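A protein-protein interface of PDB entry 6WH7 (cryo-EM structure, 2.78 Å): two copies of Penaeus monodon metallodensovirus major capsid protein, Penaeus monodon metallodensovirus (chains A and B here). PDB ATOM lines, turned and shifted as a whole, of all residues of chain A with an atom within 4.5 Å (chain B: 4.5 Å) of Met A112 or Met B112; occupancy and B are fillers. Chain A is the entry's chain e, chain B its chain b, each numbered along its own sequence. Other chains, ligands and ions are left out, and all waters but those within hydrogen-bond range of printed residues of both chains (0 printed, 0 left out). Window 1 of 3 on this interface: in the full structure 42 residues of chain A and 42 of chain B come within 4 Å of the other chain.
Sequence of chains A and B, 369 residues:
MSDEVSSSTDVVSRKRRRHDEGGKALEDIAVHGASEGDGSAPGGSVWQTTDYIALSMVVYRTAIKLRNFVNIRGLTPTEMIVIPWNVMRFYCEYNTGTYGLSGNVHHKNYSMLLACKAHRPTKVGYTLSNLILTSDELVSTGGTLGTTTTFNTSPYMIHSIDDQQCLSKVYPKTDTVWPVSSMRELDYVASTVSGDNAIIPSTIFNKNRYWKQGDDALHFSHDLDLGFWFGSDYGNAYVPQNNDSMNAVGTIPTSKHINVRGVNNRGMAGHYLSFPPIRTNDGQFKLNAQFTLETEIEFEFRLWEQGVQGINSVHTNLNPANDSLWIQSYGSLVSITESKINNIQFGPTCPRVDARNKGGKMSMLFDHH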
ATOM      1  N   LYS A 108      11.391   2.642  12.672  1.00  0.00           N
ATOM      2  CA  LYS A 108      10.988   1.719  11.623  1.00  0.00           C
ATOM      3  C   LYS A 108      10.183   2.397  10.529  1.00  0.00           C
ATOM      4  O   LYS A 108      10.170   1.903   9.400  1.00  0.00           O
ATOM      5  CB  LYS A 108      10.195   0.557  12.200  1.00  0.00           C
ATOM      6  CG  LYS A 108      11.015  -0.338  13.069  1.00  0.00           C
ATOM      7  CD  LYS A 108      10.271  -1.572  13.441  1.00  0.00           C
ATOM      8  CE  LYS A 108      10.127  -2.456  12.234  1.00  0.00           C
ATOM      9  NZ  LYS A 108      11.437  -2.931  11.742  1.00  0.00           N
ATOM     10  N   ASN A 109       9.512   3.507  10.827  1.00  0.00           N
ATOM     11  CA  ASN A 109       8.849   4.247   9.765  1.00  0.00           C
ATOM     12  C   ASN A 109       9.842   4.803   8.771  1.00  0.00           C
ATOM     13  O   ASN A 109       9.500   5.002   7.604  1.00  0.00           O
ATOM     14  CB  ASN A 109       8.003   5.379  10.332  1.00  0.00           C
ATOM     15  CG  ASN A 109       6.698   4.899  10.872  1.00  0.00           C
ATOM     16  OD1 ASN A 109       6.218   3.838  10.498  1.00  0.00           O
ATOM     17  ND2 ASN A 109       6.095   5.686  11.737  1.00  0.00           N
ATOM     18  N   TYR A 110      11.070   5.062   9.202  1.00  0.00           N
ATOM     19  CA  TYR A 110      12.043   5.565   8.251  1.00  0.00           C
ATOM     20  C   TYR A 110      12.584   4.449   7.373  1.00  0.00           C
ATOM     21  O   TYR A 110      12.700   4.619   6.157  1.00  0.00           O
ATOM     22  CB  TYR A 110      13.187   6.267   8.961  1.00  0.00           C
ATOM     23  CG  TYR A 110      14.124   6.860   7.959  1.00  0.00           C
ATOM     24  CD1 TYR A 110      13.788   8.021   7.300  1.00  0.00           C
ATOM     25  CD2 TYR A 110      15.316   6.241   7.635  1.00  0.00           C
ATOM     26  CE1 TYR A 110      14.609   8.564   6.372  1.00  0.00           C
ATOM     27  CE2 TYR A 110      16.151   6.781   6.703  1.00  0.00           C
ATOM     28  CZ  TYR A 110      15.786   7.945   6.075  1.00  0.00           C
ATOM     29  OH  TYR A 110      16.595   8.517   5.142  1.00  0.00           O
ATOM     30  N   SER A 111      12.929   3.309   7.968  1.00  0.00           N
ATOM     31  CA  SER A 111      13.368   2.166   7.179  1.00  0.00           C
ATOM     32  C   SER A 111      12.338   1.782   6.138  1.00  0.00           C
ATOM     33  O   SER A 111      12.681   1.153   5.134  1.00  0.00           O
ATOM     34  CB  SER A 111      13.652   0.980   8.092  1.00  0.00           C
ATOM     35  OG  SER A 111      14.715   1.281   8.977  1.00  0.00           O
ATOM     36  N   MET A 112      11.083   2.138   6.368  1.00  0.00           N
ATOM     37  CA  MET A 112      10.039   1.944   5.380  1.00  0.00           C
ATOM     38  C   MET A 112      10.051   3.023   4.308  1.00  0.00           C
ATOM     39  O   MET A 112       9.852   2.724   3.128  1.00  0.00           O
ATOM     40  CB  MET A 112       8.692   1.915   6.070  1.00  0.00           C
ATOM     41  CG  MET A 112       7.596   2.030   5.094  1.00  0.00           C
ATOM     42  SD  MET A 112       6.015   1.711   5.808  1.00  0.00           S
ATOM     43  CE  MET A 112       5.027   2.339   4.472  1.00  0.00           C
ATOM     44  N   LEU A 113      10.265   4.282   4.695  1.00  0.00           N
ATOM     45  CA  LEU A 113      10.392   5.354   3.716  1.00  0.00           C
ATOM     46  C   LEU A 113      11.435   5.040   2.661  1.00  0.00           C
ATOM     47  O   LEU A 113      11.344   5.551   1.542  1.00  0.00           O
ATOM     48  CB  LEU A 113      10.760   6.656   4.408  1.00  0.00           C
ATOM     49  CG  LEU A 113       9.727   7.233   5.358  1.00  0.00           C
ATOM     50  CD1 LEU A 113      10.311   8.410   6.073  1.00  0.00           C
ATOM     51  CD2 LEU A 113       8.507   7.636   4.594  1.00  0.00           C
ATOM     52  N   LEU A 114      12.425   4.225   2.998  1.00  0.00           N
ATOM     53  CA  LEU A 114      13.425   3.800   2.041  1.00  0.00           C
ATOM     54  C   LEU A 114      12.916   2.710   1.114  1.00  0.00           C
ATOM     55  O   LEU A 114      13.550   2.448   0.089  1.00  0.00           O
ATOM     56  CB  LEU A 114      14.665   3.324   2.788  1.00  0.00           C
ATOM     57  CG  LEU A 114      15.260   4.419   3.664  1.00  0.00           C
ATOM     58  CD1 LEU A 114      16.463   3.900   4.407  1.00  0.00           C
ATOM     59  CD2 LEU A 114      15.602   5.637   2.837  1.00  0.00           C
ATOM     60  N   ALA A 115      11.801   2.073   1.451  1.00  0.00           N
ATOM     61  CA  ALA A 115      11.115   1.167   0.541  1.00  0.00           C
ATOM     62  C   ALA A 115      10.128   1.888  -0.360  1.00  0.00           C
ATOM     63  O   ALA A 115       9.600   1.278  -1.291  1.00  0.00           O
ATOM     64  CB  ALA A 115      10.387   0.080   1.332  1.00  0.00           C
ATOM     65  N   CYS A 116       9.850   3.154  -0.085  1.00  0.00           N
ATOM     66  CA  CYS A 116       9.056   3.992  -0.960  1.00  0.00           C
ATOM     67  C   CYS A 116       9.876   4.395  -2.174  1.00  0.00           C
ATOM     68  O   CYS A 116      11.100   4.259  -2.199  1.00  0.00           O
ATOM     69  CB  CYS A 116       8.592   5.238  -0.224  1.00  0.00           C
ATOM     70  SG  CYS A 116       7.688   4.894   1.263  1.00  0.00           S
ATOM     71  N   PHE A 301       5.757  10.684   1.786  1.00  0.00           N
ATOM     72  CA  PHE A 301       6.331   9.691   0.903  1.00  0.00           C
ATOM     73  C   PHE A 301       5.369   9.407  -0.233  1.00  0.00           C
ATOM     74  O   PHE A 301       4.209   9.812  -0.227  1.00  0.00           O
ATOM     75  CB  PHE A 301       6.712   8.409   1.645  1.00  0.00           C
ATOM     76  CG  PHE A 301       5.575   7.724   2.326  1.00  0.00           C
ATOM     77  CD1 PHE A 301       4.880   6.718   1.695  1.00  0.00           C
ATOM     78  CD2 PHE A 301       5.210   8.075   3.609  1.00  0.00           C
ATOM     79  CE1 PHE A 301       3.855   6.078   2.329  1.00  0.00           C
ATOM     80  CE2 PHE A 301       4.179   7.442   4.241  1.00  0.00           C
ATOM     81  CZ  PHE A 301       3.505   6.441   3.609  1.00  0.00           C
ATOM     82  N   LEU A 303       4.646   6.508  -3.689  1.00  0.00           N
ATOM     83  CA  LEU A 303       4.763   5.099  -4.019  1.00  0.00           C
ATOM     84  C   LEU A 303       5.280   4.894  -5.432  1.00  0.00           C
ATOM     85  O   LEU A 303       5.535   5.834  -6.185  1.00  0.00           O
ATOM     86  CB  LEU A 303       3.424   4.392  -3.856  1.00  0.00           C
ATOM     87  CG  LEU A 303       2.890   4.461  -2.439  1.00  0.00           C
ATOM     88  CD1 LEU A 303       1.652   3.646  -2.288  1.00  0.00           C
ATOM     89  CD2 LEU A 303       3.920   3.998  -1.534  1.00  0.00           C
ATOM     90  N   LYS B 108       6.168  -3.343  -7.152  1.00  0.00           N
ATOM     91  CA  LYS B 108       7.000  -2.755  -6.114  1.00  0.00           C
ATOM     92  C   LYS B 108       6.182  -2.162  -4.981  1.00  0.00           C
ATOM     93  O   LYS B 108       6.692  -2.057  -3.864  1.00  0.00           O
ATOM     94  CB  LYS B 108       7.922  -1.694  -6.694  1.00  0.00           C
ATOM     95  CG  LYS B 108       8.960  -2.257  -7.606  1.00  0.00           C
ATOM     96  CD  LYS B 108       9.970  -1.232  -7.985  1.00  0.00           C
ATOM     97  CE  LYS B 108      10.829  -0.910  -6.795  1.00  0.00           C
ATOM     98  NZ  LYS B 108      11.617  -2.080  -6.354  1.00  0.00           N
ATOM     99  N   ASN B 109       4.937  -1.769  -5.234  1.00  0.00           N
ATOM    100  CA  ASN B 109       4.091  -1.326  -4.136  1.00  0.00           C
ATOM    101  C   ASN B 109       3.817  -2.447  -3.159  1.00  0.00           C
ATOM    102  O   ASN B 109       3.576  -2.189  -1.978  1.00  0.00           O
ATOM    103  CB  ASN B 109       2.774  -0.762  -4.651  1.00  0.00           C
ATOM    104  CG  ASN B 109       2.913   0.632  -5.162  1.00  0.00           C
ATOM    105  OD1 ASN B 109       3.840   1.342  -4.798  1.00  0.00           O
ATOM    106  ND2 ASN B 109       1.981   1.051  -5.990  1.00  0.00           N
ATOM    107  N   TYR B 110       3.845  -3.690  -3.620  1.00  0.00           N
ATOM    108  CA  TYR B 110       3.616  -4.777  -2.687  1.00  0.00           C
ATOM    109  C   TYR B 110       4.853  -5.057  -1.851  1.00  0.00           C
ATOM    110  O   TYR B 110       4.752  -5.238  -0.636  1.00  0.00           O
ATOM    111  CB  TYR B 110       3.185  -6.038  -3.415  1.00  0.00           C
ATOM    112  CG  TYR B 110       2.863  -7.113  -2.428  1.00  0.00           C
ATOM    113  CD1 TYR B 110       1.674  -7.080  -1.733  1.00  0.00           C
ATOM    114  CD2 TYR B 110       3.756  -8.131  -2.154  1.00  0.00           C
ATOM    115  CE1 TYR B 110       1.370  -8.028  -0.818  1.00  0.00           C
ATOM    116  CE2 TYR B 110       3.458  -9.092  -1.235  1.00  0.00           C
ATOM    117  CZ  TYR B 110       2.260  -9.030  -0.570  1.00  0.00           C
ATOM    118  OH  TYR B 110       1.924  -9.974   0.351  1.00  0.00           O
ATOM    119  N   SER B 111       6.025  -5.107  -2.483  1.00  0.00           N
ATOM    120  CA  SER B 111       7.262  -5.278  -1.734  1.00  0.00           C
ATOM    121  C   SER B 111       7.421  -4.211  -0.671  1.00  0.00           C
ATOM    122  O   SER B 111       8.143  -4.418   0.307  1.00  0.00           O
ATOM    123  CB  SER B 111       8.454  -5.249  -2.682  1.00  0.00           C
ATOM    124  OG  SER B 111       8.389  -6.332  -3.591  1.00  0.00           O
ATOM    125  N   MET B 112       6.770  -3.071  -0.855  1.00  0.00           N
ATOM    126  CA  MET B 112       6.739  -2.035   0.158  1.00  0.00           C
ATOM    127  C   MET B 112       5.726  -2.329   1.255  1.00  0.00           C
ATOM    128  O   MET B 112       6.004  -2.092   2.433  1.00  0.00           O
ATOM    129  CB  MET B 112       6.426  -0.704  -0.491  1.00  0.00           C
ATOM    130  CG  MET B 112       6.082   0.310   0.518  1.00  0.00           C
ATOM    131  SD  MET B 112       5.995   1.937  -0.154  1.00  0.00           S
ATOM    132  CE  MET B 112       5.189   2.715   1.224  1.00  0.00           C
ATOM    133  N   LEU B 113       4.544  -2.828   0.890  1.00  0.00           N
ATOM    134  CA  LEU B 113       3.562  -3.231   1.889  1.00  0.00           C
ATOM    135  C   LEU B 113       4.145  -4.193   2.905  1.00  0.00           C
ATOM    136  O   LEU B 113       3.661  -4.253   4.037  1.00  0.00           O
ATOM    137  CB  LEU B 113       2.364  -3.883   1.217  1.00  0.00           C
ATOM    138  CG  LEU B 113       1.530  -2.994   0.310  1.00  0.00           C
ATOM    139  CD1 LEU B 113       0.506  -3.826  -0.393  1.00  0.00           C
ATOM    140  CD2 LEU B 113       0.871  -1.924   1.121  1.00  0.00           C
ATOM    141  N   LEU B 114       5.162  -4.951   2.521  1.00  0.00           N
ATOM    142  CA  LEU B 114       5.841  -5.843   3.437  1.00  0.00           C
ATOM    143  C   LEU B 114       6.805  -5.111   4.353  1.00  0.00           C
ATOM    144  O   LEU B 114       7.241  -5.688   5.352  1.00  0.00           O
ATOM    145  CB  LEU B 114       6.577  -6.916   2.643  1.00  0.00           C
ATOM    146  CG  LEU B 114       5.629  -7.734   1.775  1.00  0.00           C
ATOM    147  CD1 LEU B 114       6.398  -8.761   0.984  1.00  0.00           C
ATOM    148  CD2 LEU B 114       4.553  -8.377   2.617  1.00  0.00           C
ATOM    149  N   ALA B 115       7.149  -3.867   4.036  1.00  0.00           N
ATOM    150  CA  ALA B 115       7.891  -3.008   4.943  1.00  0.00           C
ATOM    151  C   ALA B 115       6.982  -2.243   5.890  1.00  0.00           C
ATOM    152  O   ALA B 115       7.477  -1.607   6.823  1.00  0.00           O
ATOM    153  CB  ALA B 115       8.751  -2.023   4.151  1.00  0.00           C
ATOM    154  N   CYS B 116       5.680  -2.269   5.652  1.00  0.00           N
ATOM    155  CA  CYS B 116       4.704  -1.718   6.570  1.00  0.00           C
ATOM    156  C   CYS B 116       4.543  -2.640   7.768  1.00  0.00           C
ATOM    157  O   CYS B 116       4.966  -3.795   7.754  1.00  0.00           O
ATOM    158  CB  CYS B 116       3.361  -1.548   5.877  1.00  0.00           C
ATOM    159  SG  CYS B 116       3.437  -0.553   4.410  1.00  0.00           S
ATOM    160  N   PHE B 301      -2.659  -0.049   4.078  1.00  0.00           N
ATOM    161  CA  PHE B 301      -1.534  -0.389   4.921  1.00  0.00           C
ATOM    162  C   PHE B 301      -1.452   0.585   6.078  1.00  0.00           C
ATOM    163  O   PHE B 301      -2.122   1.616   6.115  1.00  0.00           O
ATOM    164  CB  PHE B 301      -0.218  -0.435   4.139  1.00  0.00           C
ATOM    165  CG  PHE B 301       0.155   0.848   3.476  1.00  0.00           C
ATOM    166  CD1 PHE B 301       0.984   1.748   4.104  1.00  0.00           C
ATOM    167  CD2 PHE B 301      -0.310   1.147   2.214  1.00  0.00           C
ATOM    168  CE1 PHE B 301       1.343   2.911   3.487  1.00  0.00           C
ATOM    169  CE2 PHE B 301       0.040   2.314   1.597  1.00  0.00           C
ATOM    170  CZ  PHE B 301       0.870   3.194   2.227  1.00  0.00           C
ATOM    171  N   LEU B 303       1.292   1.899   9.486  1.00  0.00           N
ATOM    172  CA  LEU B 303       2.696   2.114   9.781  1.00  0.00           C
ATOM    173  C   LEU B 303       3.060   1.628  11.173  1.00  0.00           C
ATOM    174  O   LEU B 303       2.231   1.138  11.938  1.00  0.00           O
ATOM    175  CB  LEU B 303       3.060   3.587   9.641  1.00  0.00           C
ATOM    176  CG  LEU B 303       2.824   4.121   8.243  1.00  0.00           C
ATOM    177  CD1 LEU B 303       3.316   5.521   8.110  1.00  0.00           C
ATOM    178  CD2 LEU B 303       3.493   3.253   7.297  1.00  0.00           C
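The side-chain sulfur (SG) of Cys A116 sits close to the side-chain sulfur (SD) of Met B112, at 3.7 Å.
SD of Met A112 sits close to SG of Cys B116.
SD of Met A112 sits close to O of Ala B115, 3.8 Å away.
The backbone carbonyl oxygen of Met B112 is in hydrogen-bond range of the side-chain sulfur of Cys B116.
SG of Cys A116 lies close to O of Leu A113, 3.7 Å away.
The backbone carbonyl oxygen (O) of Met A112 lies within hydrogen-bond range of the side-chain sulfur (SG) of Cys A116, at 3.6 Å.
SG of Cys B116 sits close to O of Leu B113, at 3.7 Å.
Leu B303 touches Asn A109.
CE of Met B112 touches CE of Met A112 (3.3 Å).
Met A112 touches Phe B301.
Met A112 touches Leu B303 (SD to CD2, 3.3 Å).
Met B112 touches Ala A115 (CB to O, 3.8 Å).
CB of Ala A115 touches CB of Ala B115, 3.9 Å away.
Phe A301 touches Met B112.
Asn B109 touches Leu A303 (OD1 to CB, 3.2 Å).
CD2 of Leu A303 touches SD of Met B112, 3.2 Å away.
Ser A111 touches none of the printed residues of chain B.
Of chain B, only Met B112 (3.3 Å), Ala B115 (3.8 Å), Cys B116 (3.3 Å), Phe B301 (3.9 Å) and Leu B303 (3.3 Å) come within 4 Å of Met A112.
Printed residues of chain B within 4 Å of Phe A301: Met B112.
Met B112 touches just these residues of chain A: Met A112 (3.3 Å), Ala A115 (3.8 Å), Cys A116 (3.3 Å), Phe A301 (3.8 Å) and Leu A303 (3.2 Å).
Of the printed residues of chain A, Ala B115 touches Met A112 (3.8 Å) and Ala A115 (3.9 Å).
Of the printed residues of chain A, Cys B116 touches Met A112 (3.3 Å).
The nearest printed residue of chain B that does not touch Met A112 is Leu B113 (6.3 Å).
Printed residues of chain A that touch a printed residue of chain B: Asn A109, Met A112, Ala A115, Cys A116, Phe A301 and Leu A303.
Of the 11 printed residues of chain B, 6 touch a printed residue of chain A.
Printed residues of chain B that touch a printed residue of chain A: Asn B109, Met B112, Ala B115, Cys B116, Phe B301 and Leu B303.
Among the printed residues, 12 pairs touch across the chains.
Among the printed residues, no Asp or Glu carboxylate lies within 4 Å of a Lys or Arg side-chain nitrogen of the other chain.
Met B112 touches its own counterpart, Met A112.
Met A112 touches Cys B116, and with the chains exchanged Cys A116 touches Met B112.
Met A112 touches Phe B301, and with the chains exchanged Phe A301 touches Met B112.
Ala A115 touches its own counterpart, Ala B115.
Positions printed for both chains: 108, 109, 110, 111, 112, 113, 114, 115, 116, 301 and 303.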
